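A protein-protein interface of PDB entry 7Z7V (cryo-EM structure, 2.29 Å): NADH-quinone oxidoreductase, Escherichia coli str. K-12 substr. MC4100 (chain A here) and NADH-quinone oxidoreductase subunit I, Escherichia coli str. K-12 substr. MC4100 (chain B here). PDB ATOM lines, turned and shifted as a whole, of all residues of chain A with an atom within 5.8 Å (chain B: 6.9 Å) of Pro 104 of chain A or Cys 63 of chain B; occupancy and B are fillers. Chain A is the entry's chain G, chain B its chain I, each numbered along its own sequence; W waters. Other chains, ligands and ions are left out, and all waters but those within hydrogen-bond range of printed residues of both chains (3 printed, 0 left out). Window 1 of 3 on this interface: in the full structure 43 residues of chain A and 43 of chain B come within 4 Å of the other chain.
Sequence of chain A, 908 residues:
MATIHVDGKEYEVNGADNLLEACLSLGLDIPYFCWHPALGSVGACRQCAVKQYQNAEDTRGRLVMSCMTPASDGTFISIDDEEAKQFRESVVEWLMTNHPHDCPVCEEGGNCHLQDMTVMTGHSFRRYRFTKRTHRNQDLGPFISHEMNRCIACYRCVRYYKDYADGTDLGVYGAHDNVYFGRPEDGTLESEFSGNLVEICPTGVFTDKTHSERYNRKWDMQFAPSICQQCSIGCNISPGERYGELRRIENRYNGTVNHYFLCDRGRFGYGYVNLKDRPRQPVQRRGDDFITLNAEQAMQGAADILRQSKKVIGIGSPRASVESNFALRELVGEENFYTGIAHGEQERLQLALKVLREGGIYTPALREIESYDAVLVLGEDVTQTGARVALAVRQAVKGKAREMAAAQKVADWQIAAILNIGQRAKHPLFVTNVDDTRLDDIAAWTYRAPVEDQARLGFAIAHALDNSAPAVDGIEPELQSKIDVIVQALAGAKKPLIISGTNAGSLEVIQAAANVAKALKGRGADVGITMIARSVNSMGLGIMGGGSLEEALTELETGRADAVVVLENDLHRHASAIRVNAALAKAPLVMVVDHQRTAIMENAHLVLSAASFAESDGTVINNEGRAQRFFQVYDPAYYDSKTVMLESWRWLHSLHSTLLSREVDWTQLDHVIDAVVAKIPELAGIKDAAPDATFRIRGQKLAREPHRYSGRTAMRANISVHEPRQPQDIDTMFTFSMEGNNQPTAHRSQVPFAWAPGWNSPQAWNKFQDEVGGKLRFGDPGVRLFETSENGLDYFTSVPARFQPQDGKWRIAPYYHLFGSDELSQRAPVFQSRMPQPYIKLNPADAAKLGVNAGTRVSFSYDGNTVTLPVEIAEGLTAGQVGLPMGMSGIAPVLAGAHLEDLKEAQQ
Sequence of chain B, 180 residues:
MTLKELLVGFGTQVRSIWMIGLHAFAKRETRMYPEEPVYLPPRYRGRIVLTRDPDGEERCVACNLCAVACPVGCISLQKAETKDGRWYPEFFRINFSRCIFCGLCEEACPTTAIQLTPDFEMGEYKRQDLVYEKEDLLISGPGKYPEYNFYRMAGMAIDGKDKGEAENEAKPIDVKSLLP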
ATOM      1  N   HIS A 101      27.251   1.722  19.628  1.00  0.00           N
ATOM      2  CA  HIS A 101      26.782   2.340  20.870  1.00  0.00           C
ATOM      3  C   HIS A 101      25.804   1.385  21.562  1.00  0.00           C
ATOM      4  O   HIS A 101      24.608   1.643  21.691  1.00  0.00           O
ATOM      5  CB  HIS A 101      26.139   3.682  20.545  1.00  0.00           C
ATOM      6  CG  HIS A 101      25.982   4.596  21.718  1.00  0.00           C
ATOM      7  ND1 HIS A 101      26.951   5.500  22.093  1.00  0.00           N
ATOM      8  CD2 HIS A 101      24.954   4.769  22.581  1.00  0.00           C
ATOM      9  CE1 HIS A 101      26.534   6.178  23.145  1.00  0.00           C
ATOM     10  NE2 HIS A 101      25.324   5.754  23.460  1.00  0.00           N
ATOM     11  N   ASP A 102      26.341   0.256  22.025  1.00  0.00           N
ATOM     12  CA  ASP A 102      25.517  -0.911  22.292  1.00  0.00           C
ATOM     13  C   ASP A 102      25.509  -1.406  23.732  1.00  0.00           C
ATOM     14  O   ASP A 102      24.708  -2.294  24.030  1.00  0.00           O
ATOM     15  CB  ASP A 102      25.950  -2.082  21.394  1.00  0.00           C
ATOM     16  CG  ASP A 102      25.104  -2.220  20.157  1.00  0.00           C
ATOM     17  OD1 ASP A 102      24.375  -1.272  19.816  1.00  0.00           O
ATOM     18  OD2 ASP A 102      25.177  -3.286  19.518  1.00  0.00           O
ATOM     19  N   CYS A 103      26.357  -0.869  24.617  1.00  0.00           N
ATOM     20  CA  CYS A 103      26.508  -1.409  25.974  1.00  0.00           C
ATOM     21  C   CYS A 103      25.212  -1.596  26.769  1.00  0.00           C
ATOM     22  O   CYS A 103      25.100  -2.628  27.449  1.00  0.00           O
ATOM     23  CB  CYS A 103      27.464  -0.535  26.802  1.00  0.00           C
ATOM     24  SG  CYS A 103      29.141  -0.365  26.222  1.00  0.00           S
ATOM     25  N   PRO A 104      24.226  -0.681  26.754  1.00  0.00           N
ATOM     26  CA  PRO A 104      22.967  -0.984  27.457  1.00  0.00           C
ATOM     27  C   PRO A 104      22.213  -2.192  26.923  1.00  0.00           C
ATOM     28  O   PRO A 104      21.498  -2.844  27.689  1.00  0.00           O
ATOM     29  CB  PRO A 104      22.153   0.302  27.277  1.00  0.00           C
ATOM     30  CG  PRO A 104      23.146   1.336  27.071  1.00  0.00           C
ATOM     31  CD  PRO A 104      24.212   0.713  26.272  1.00  0.00           C
ATOM     32  N   VAL A 105      22.340  -2.515  25.641  1.00  0.00           N
ATOM     33  CA  VAL A 105      21.583  -3.625  25.072  1.00  0.00           C
ATOM     34  C   VAL A 105      22.522  -4.753  24.676  1.00  0.00           C
ATOM     35  O   VAL A 105      22.229  -5.528  23.763  1.00  0.00           O
ATOM     36  CB  VAL A 105      20.745  -3.165  23.870  1.00  0.00           C
ATOM     37  CG1 VAL A 105      19.543  -2.399  24.342  1.00  0.00           C
ATOM     38  CG2 VAL A 105      21.581  -2.325  22.920  1.00  0.00           C
ATOM     39  N   CYS A 106      23.653  -4.854  25.358  1.00  0.00           N
ATOM     40  CA  CYS A 106      24.664  -5.849  25.048  1.00  0.00           C
ATOM     41  C   CYS A 106      24.845  -6.765  26.244  1.00  0.00           C
ATOM     42  O   CYS A 106      25.051  -6.295  27.366  1.00  0.00           O
ATOM     43  CB  CYS A 106      25.981  -5.181  24.682  1.00  0.00           C
ATOM     44  SG  CYS A 106      27.327  -6.274  24.270  1.00  0.00           S
ATOM     45  N   ARG A 217      22.700  -8.880  34.612  1.00  0.00           N
ATOM     46  CA  ARG A 217      24.103  -8.508  34.609  1.00  0.00           C
ATOM     47  C   ARG A 217      24.882  -9.313  35.645  1.00  0.00           C
ATOM     48  O   ARG A 217      24.312  -9.936  36.543  1.00  0.00           O
ATOM     49  CB  ARG A 217      24.249  -7.013  34.867  1.00  0.00           C
ATOM     50  CG  ARG A 217      23.461  -6.167  33.890  1.00  0.00           C
ATOM     51  CD  ARG A 217      24.305  -5.800  32.700  1.00  0.00           C
ATOM     52  NE  ARG A 217      23.611  -4.905  31.787  1.00  0.00           N
ATOM     53  CZ  ARG A 217      23.854  -4.830  30.487  1.00  0.00           C
ATOM     54  NH1 ARG A 217      24.771  -5.587  29.913  1.00  0.00           N
ATOM     55  NH2 ARG A 217      23.160  -3.977  29.746  1.00  0.00           N
ATOM     56  N   TRP A 219      26.925  -8.366  38.056  1.00  0.00           N
ATOM     57  CA  TRP A 219      26.860  -7.878  39.428  1.00  0.00           C
ATOM     58  C   TRP A 219      25.573  -8.285  40.135  1.00  0.00           C
ATOM     59  O   TRP A 219      25.543  -8.306  41.366  1.00  0.00           O
ATOM     60  CB  TRP A 219      27.016  -6.354  39.463  1.00  0.00           C
ATOM     61  CG  TRP A 219      26.003  -5.594  38.649  1.00  0.00           C
ATOM     62  CD1 TRP A 219      24.697  -5.375  38.963  1.00  0.00           C
ATOM     63  CD2 TRP A 219      26.225  -4.943  37.395  1.00  0.00           C
ATOM     64  NE1 TRP A 219      24.089  -4.645  37.980  1.00  0.00           N
ATOM     65  CE2 TRP A 219      25.008  -4.355  37.010  1.00  0.00           C
ATOM     66  CE3 TRP A 219      27.335  -4.800  36.561  1.00  0.00           C
ATOM     67  CZ2 TRP A 219      24.870  -3.634  35.830  1.00  0.00           C
ATOM     68  CZ3 TRP A 219      27.192  -4.093  35.386  1.00  0.00           C
ATOM     69  CH2 TRP A 219      25.968  -3.522  35.029  1.00  0.00           C
ATOM     70  N   CYS B  60      12.990   2.516  28.111  1.00  0.00           N
ATOM     71  CA  CYS B  60      13.803   1.636  28.937  1.00  0.00           C
ATOM     72  C   CYS B  60      14.197   0.384  28.171  1.00  0.00           C
ATOM     73  O   CYS B  60      13.350  -0.320  27.618  1.00  0.00           O
ATOM     74  CB  CYS B  60      13.064   1.260  30.214  1.00  0.00           C
ATOM     75  SG  CYS B  60      14.009   0.145  31.253  1.00  0.00           S
ATOM     76  N   VAL B  61      15.498   0.118  28.134  1.00  0.00           N
ATOM     77  CA  VAL B  61      16.030  -1.059  27.474  1.00  0.00           C
ATOM     78  C   VAL B  61      16.419  -2.132  28.477  1.00  0.00           C
ATOM     79  O   VAL B  61      17.078  -3.105  28.111  1.00  0.00           O
ATOM     80  CB  VAL B  61      17.215  -0.689  26.574  1.00  0.00           C
ATOM     81  CG1 VAL B  61      16.787   0.335  25.549  1.00  0.00           C
ATOM     82  CG2 VAL B  61      18.377  -0.170  27.404  1.00  0.00           C
ATOM     83  N   ALA B  62      16.030  -1.960  29.744  1.00  0.00           N
ATOM     84  CA  ALA B  62      16.276  -2.917  30.822  1.00  0.00           C
ATOM     85  C   ALA B  62      17.760  -3.235  30.970  1.00  0.00           C
ATOM     86  O   ALA B  62      18.157  -4.383  31.161  1.00  0.00           O
ATOM     87  CB  ALA B  62      15.454  -4.189  30.630  1.00  0.00           C
ATOM     88  N   CYS B  63      18.586  -2.200  30.871  1.00  0.00           N
ATOM     89  CA  CYS B  63      20.025  -2.357  30.975  1.00  0.00           C
ATOM     90  C   CYS B  63      20.505  -2.525  32.409  1.00  0.00           C
ATOM     91  O   CYS B  63      21.670  -2.885  32.607  1.00  0.00           O
ATOM     92  CB  CYS B  63      20.711  -1.159  30.331  1.00  0.00           C
ATOM     93  SG  CYS B  63      20.799   0.296  31.351  1.00  0.00           S
ATOM     94  N   ASN B  64      19.641  -2.261  33.390  1.00  0.00           N
ATOM     95  CA  ASN B  64      19.874  -2.444  34.822  1.00  0.00           C
ATOM     96  C   ASN B  64      20.956  -1.533  35.388  1.00  0.00           C
ATOM     97  O   ASN B  64      21.506  -1.825  36.448  1.00  0.00           O
ATOM     98  CB  ASN B  64      20.195  -3.905  35.165  1.00  0.00           C
ATOM     99  CG  ASN B  64      19.047  -4.607  35.840  1.00  0.00           C
ATOM    100  OD1 ASN B  64      18.757  -4.359  37.003  1.00  0.00           O
ATOM    101  ND2 ASN B  64      18.382  -5.486  35.110  1.00  0.00           N
ATOM    102  N   LEU B  65      21.260  -0.415  34.728  1.00  0.00           N
ATOM    103  CA  LEU B  65      22.245   0.506  35.288  1.00  0.00           C
ATOM    104  C   LEU B  65      21.666   1.314  36.445  1.00  0.00           C
ATOM    105  O   LEU B  65      22.380   1.622  37.404  1.00  0.00           O
ATOM    106  CB  LEU B  65      22.779   1.439  34.201  1.00  0.00           C
ATOM    107  CG  LEU B  65      23.866   0.913  33.255  1.00  0.00           C
ATOM    108  CD1 LEU B  65      24.416   2.044  32.405  1.00  0.00           C
ATOM    109  CD2 LEU B  65      24.987   0.197  33.995  1.00  0.00           C
ATOM    110  N   CYS B  66      20.379   1.667  36.371  1.00  0.00           N
ATOM    111  CA  CYS B  66      19.750   2.424  37.448  1.00  0.00           C
ATOM    112  C   CYS B  66      19.683   1.616  38.736  1.00  0.00           C
ATOM    113  O   CYS B  66      19.882   2.163  39.824  1.00  0.00           O
ATOM    114  CB  CYS B  66      18.346   2.865  37.042  1.00  0.00           C
ATOM    115  SG  CYS B  66      17.248   1.532  36.547  1.00  0.00           S
ATOM    116  N   VAL B  68      21.669  -0.863  39.799  1.00  0.00           N
ATOM    117  CA  VAL B  68      22.964  -0.997  40.454  1.00  0.00           C
ATOM    118  C   VAL B  68      23.480   0.362  40.923  1.00  0.00           C
ATOM    119  O   VAL B  68      24.185   0.445  41.932  1.00  0.00           O
ATOM    120  CB  VAL B  68      23.957  -1.725  39.526  1.00  0.00           C
ATOM    121  CG1 VAL B  68      24.197  -0.953  38.250  1.00  0.00           C
ATOM    122  CG2 VAL B  68      25.260  -2.050  40.242  1.00  0.00           C
ATOM    123  N   LEU B  77      14.135  -4.966  38.302  1.00  0.00           N
ATOM    124  CA  LEU B  77      13.596  -5.106  36.956  1.00  0.00           C
ATOM    125  C   LEU B  77      14.201  -6.340  36.299  1.00  0.00           C
ATOM    126  O   LEU B  77      15.175  -6.913  36.787  1.00  0.00           O
ATOM    127  CB  LEU B  77      13.862  -3.849  36.126  1.00  0.00           C
ATOM    128  CG  LEU B  77      15.333  -3.559  35.832  1.00  0.00           C
ATOM    129  CD1 LEU B  77      15.574  -3.627  34.351  1.00  0.00           C
ATOM    130  CD2 LEU B  77      15.756  -2.213  36.388  1.00  0.00           C
ATOM    131  N   LYS B  79      15.051  -7.954  32.209  1.00  0.00           N
ATOM    132  CA  LYS B  79      15.084  -7.758  30.769  1.00  0.00           C
ATOM    133  C   LYS B  79      14.192  -8.765  30.054  1.00  0.00           C
ATOM    134  O   LYS B  79      14.120  -9.937  30.428  1.00  0.00           O
ATOM    135  CB  LYS B  79      16.525  -7.865  30.265  1.00  0.00           C
ATOM    136  CG  LYS B  79      16.710  -7.674  28.769  1.00  0.00           C
ATOM    137  CD  LYS B  79      17.081  -8.983  28.107  1.00  0.00           C
ATOM    138  CE  LYS B  79      16.851  -8.961  26.620  1.00  0.00           C
ATOM    139  NZ  LYS B  79      17.204 -10.264  26.012  1.00  0.00           N
ATOM    140  N   TRP B  87      15.113  -4.664  23.393  1.00  0.00           N
ATOM    141  CA  TRP B  87      15.131  -4.897  24.829  1.00  0.00           C
ATOM    142  C   TRP B  87      14.134  -3.977  25.525  1.00  0.00           C
ATOM    143  O   TRP B  87      13.979  -2.813  25.149  1.00  0.00           O
ATOM    144  CB  TRP B  87      16.526  -4.649  25.391  1.00  0.00           C
ATOM    145  CG  TRP B  87      17.570  -5.671  25.070  1.00  0.00           C
ATOM    146  CD1 TRP B  87      17.651  -6.448  23.954  1.00  0.00           C
ATOM    147  CD2 TRP B  87      18.701  -6.007  25.875  1.00  0.00           C
ATOM    148  NE1 TRP B  87      18.757  -7.251  24.017  1.00  0.00           N
ATOM    149  CE2 TRP B  87      19.421  -6.999  25.187  1.00  0.00           C
ATOM    150  CE3 TRP B  87      19.176  -5.566  27.113  1.00  0.00           C
ATOM    151  CZ2 TRP B  87      20.583  -7.561  25.698  1.00  0.00           C
ATOM    152  CZ3 TRP B  87      20.329  -6.124  27.617  1.00  0.00           C
ATOM    153  CH2 TRP B  87      21.023  -7.110  26.910  1.00  0.00           C
ATOM    154  N   ALA B 108      22.417   7.811  36.014  1.00  0.00           N
ATOM    155  CA  ALA B 108      23.025   6.627  35.426  1.00  0.00           C
ATOM    156  C   ALA B 108      22.299   6.107  34.194  1.00  0.00           C
ATOM    157  O   ALA B 108      22.855   5.256  33.498  1.00  0.00           O
ATOM    158  CB  ALA B 108      23.101   5.511  36.456  1.00  0.00           C
ATOM    159  N   CYS B 109      21.095   6.584  33.905  1.00  0.00           N
ATOM    160  CA  CYS B 109      20.327   6.042  32.789  1.00  0.00           C
ATOM    161  C   CYS B 109      20.928   6.467  31.460  1.00  0.00           C
ATOM    162  O   CYS B 109      21.017   7.668  31.189  1.00  0.00           O
ATOM    163  CB  CYS B 109      18.873   6.485  32.854  1.00  0.00           C
ATOM    164  SG  CYS B 109      17.773   5.705  31.639  1.00  0.00           S
ATOM    165  N   PRO B 110      21.327   5.532  30.604  1.00  0.00           N
ATOM    166  CA  PRO B 110      21.890   5.883  29.297  1.00  0.00           C
ATOM    167  C   PRO B 110      20.863   6.074  28.194  1.00  0.00           C
ATOM    168  O   PRO B 110      21.253   6.325  27.052  1.00  0.00           O
ATOM    169  CB  PRO B 110      22.783   4.675  28.999  1.00  0.00           C
ATOM    170  CG  PRO B 110      22.105   3.543  29.685  1.00  0.00           C
ATOM    171  CD  PRO B 110      21.289   4.076  30.817  1.00  0.00           C
ATOM    172  N   THR B 111      19.575   5.939  28.491  1.00  0.00           N
ATOM    173  CA  THR B 111      18.525   6.175  27.513  1.00  0.00           C
ATOM    174  C   THR B 111      17.602   7.319  27.902  1.00  0.00           C
ATOM    175  O   THR B 111      16.682   7.629  27.140  1.00  0.00           O
ATOM    176  CB  THR B 111      17.684   4.906  27.302  1.00  0.00           C
ATOM    177  OG1 THR B 111      16.794   4.737  28.408  1.00  0.00           O
ATOM    178  CG2 THR B 111      18.555   3.671  27.177  1.00  0.00           C
ATOM    179  N   PHE B 150      17.631   6.405  22.273  1.00  0.00           N
ATOM    180  CA  PHE B 150      18.827   5.574  22.372  1.00  0.00           C
ATOM    181  C   PHE B 150      18.955   4.648  21.173  1.00  0.00           C
ATOM    182  O   PHE B 150      20.062   4.422  20.671  1.00  0.00           O
ATOM    183  CB  PHE B 150      18.804   4.756  23.663  1.00  0.00           C
ATOM    184  CG  PHE B 150      19.797   3.624  23.683  1.00  0.00           C
ATOM    185  CD1 PHE B 150      21.142   3.875  23.882  1.00  0.00           C
ATOM    186  CD2 PHE B 150      19.388   2.313  23.490  1.00  0.00           C
ATOM    187  CE1 PHE B 150      22.059   2.845  23.895  1.00  0.00           C
ATOM    188  CE2 PHE B 150      20.300   1.280  23.498  1.00  0.00           C
ATOM    189  CZ  PHE B 150      21.638   1.547  23.700  1.00  0.00           C
ATOM    190  N   ALA B 154      22.127   3.140  18.878  1.00  0.00           N
ATOM    191  CA  ALA B 154      22.640   1.795  19.071  1.00  0.00           C
ATOM    192  C   ALA B 154      22.855   1.091  17.739  1.00  0.00           C
ATOM    193  O   ALA B 154      22.138   1.321  16.766  1.00  0.00           O
ATOM    194  CB  ALA B 154      21.681   0.980  19.937  1.00  0.00           C
HETATM  195  O   HOH W   1      23.149   6.274  25.273  1.00  0.00           O
HETATM  196  O   HOH W   2      20.685  -7.372  36.035  1.00  0.00           O
HETATM  197  O   HOH W   3      21.403  -3.913  38.362  1.00  0.00           O
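O of Cys 63 of chain B sits at hydrogen-bond distance from NE of Arg 217 of chain A.
NH1 of Arg 217 of chain A lies within hydrogen-bond range of O of Cys 106 of chain A (2.7 Å). SG of Cys 63 of chain B sits close to N of Leu 65 of chain B (3.5 Å). NH2 of Arg 217 of chain A is in hydrogen-bond range of O of Cys 103 of chain A (3.3 Å). The guanidinium group of Arg 217 of chain A lies within hydrogen-bond range of the backbone carbonyl oxygen of Pro 104 of chain A, at 2.9 Å.
Among the printed residues, pairs that only touch across the chains: His 101 of chain A with Phe 150 of chain B (3.6 Å), His 101 of chain A with Ala 154 of chain B (3.3 Å), Asp 102 of chain A with Ala 154 of chain B (3.5 Å), Pro 104 of chain A with Val 61 of chain B (3.8 Å), Pro 104 of chain A with Cys 63 of chain B (3.2 Å), Pro 104 of chain A with Trp 87 of chain B (3.5 Å), Pro 104 of chain A with Pro 110 of chain B (3.6 Å), Pro 104 of chain A with Phe 150 of chain B (3.7 Å), Val 105 of chain A with Val 61 of chain B (3.7 Å), Val 105 of chain A with Trp 87 of chain B (3.3 Å), Val 105 of chain A with Phe 150 of chain B (3.8 Å), Cys 106 of chain A with Trp 87 of chain B (3.8 Å), Trp 219 of chain A with Asn 64 of chain B (3.9 Å), Trp 219 of chain A with Leu 65 of chain B (3.98 Å) and Trp 219 of chain A with Val 68 of chain B (3.3 Å).
Of the printed residues of chain A, Pro 110 of chain B touches Pro 104. Printed residues of chain A within 4 Å of Val 61 of chain B: Pro 104 and Val 105. Printed residues of chain A within 4 Å of Val 68 of chain B: Trp 219 (3.3 Å). Of the printed residues of chain B, Arg 217 of chain A touches Cys 63. Printed residues of chain A within 4 Å of Leu 65 of chain B: Trp 219 (3.98 Å). Cys 60 of chain B touches none of the printed residues of chain A. The nearest residue of chain B that does not touch Pro 104 of chain A is Thr 111 of chain B (4.9 Å). The nearest residue of chain A that does not touch Cys 63 of chain B is Trp 219 of chain A (4.6 Å). The nearest printed residue of chain B that does not touch Cys 106 of chain A is Cys 63 of chain B (6.9 Å).
Of the 17 printed residues of chain B, 9 touch a printed residue of chain A. Printed residues of chain B that touch a printed residue of chain A: Val 61, Cys 63, Asn 64, Leu 65, Val 68, Trp 87, Pro 110, Phe 150 and Ala 154. Hydrophobic or aromatic side chains of chain B within 4 Å of the printed part of chain A: Val 61, Leu 65, Val 68, Trp 87, Pro 110, Phe 150 and Ala 154. Of the 8 printed residues of chain A, 7 touch a printed residue of chain B. Printed residues of chain A that touch a printed residue of chain B: His 101, Asp 102, Pro 104, Val 105, Cys 106, Arg 217 and Trp 219. Hydrophobic or aromatic side chains of chain A within 4 Å of the printed part of chain B: His 101, Pro 104, Val 105 and Trp 219. Along chain A the printed residues that touch a printed residue of chain B span positions 101 to 219. Among the printed residues, 16 pairs touch across the chains. Among the printed residues, no Asp or Glu carboxylate lies within 4 Å of a Lys or Arg side-chain nitrogen of the other chain.
Water W1 lies within hydrogen-bond range of O of Pro 110 of chain B (2.6 Å) and NE2 of His 101 of chain A (2.9 Å). Water W3 lies within hydrogen-bond range of NE1 of Trp 219 of chain A, O of Asn 64 of chain B and N of Val 68 of chain B. Water W2 lies within hydrogen-bond range of the backbone NH of Arg 217 of chain A (2.9 Å) and the side-chain amide nitrogen of Asn 64 of chain B (3.1 Å).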
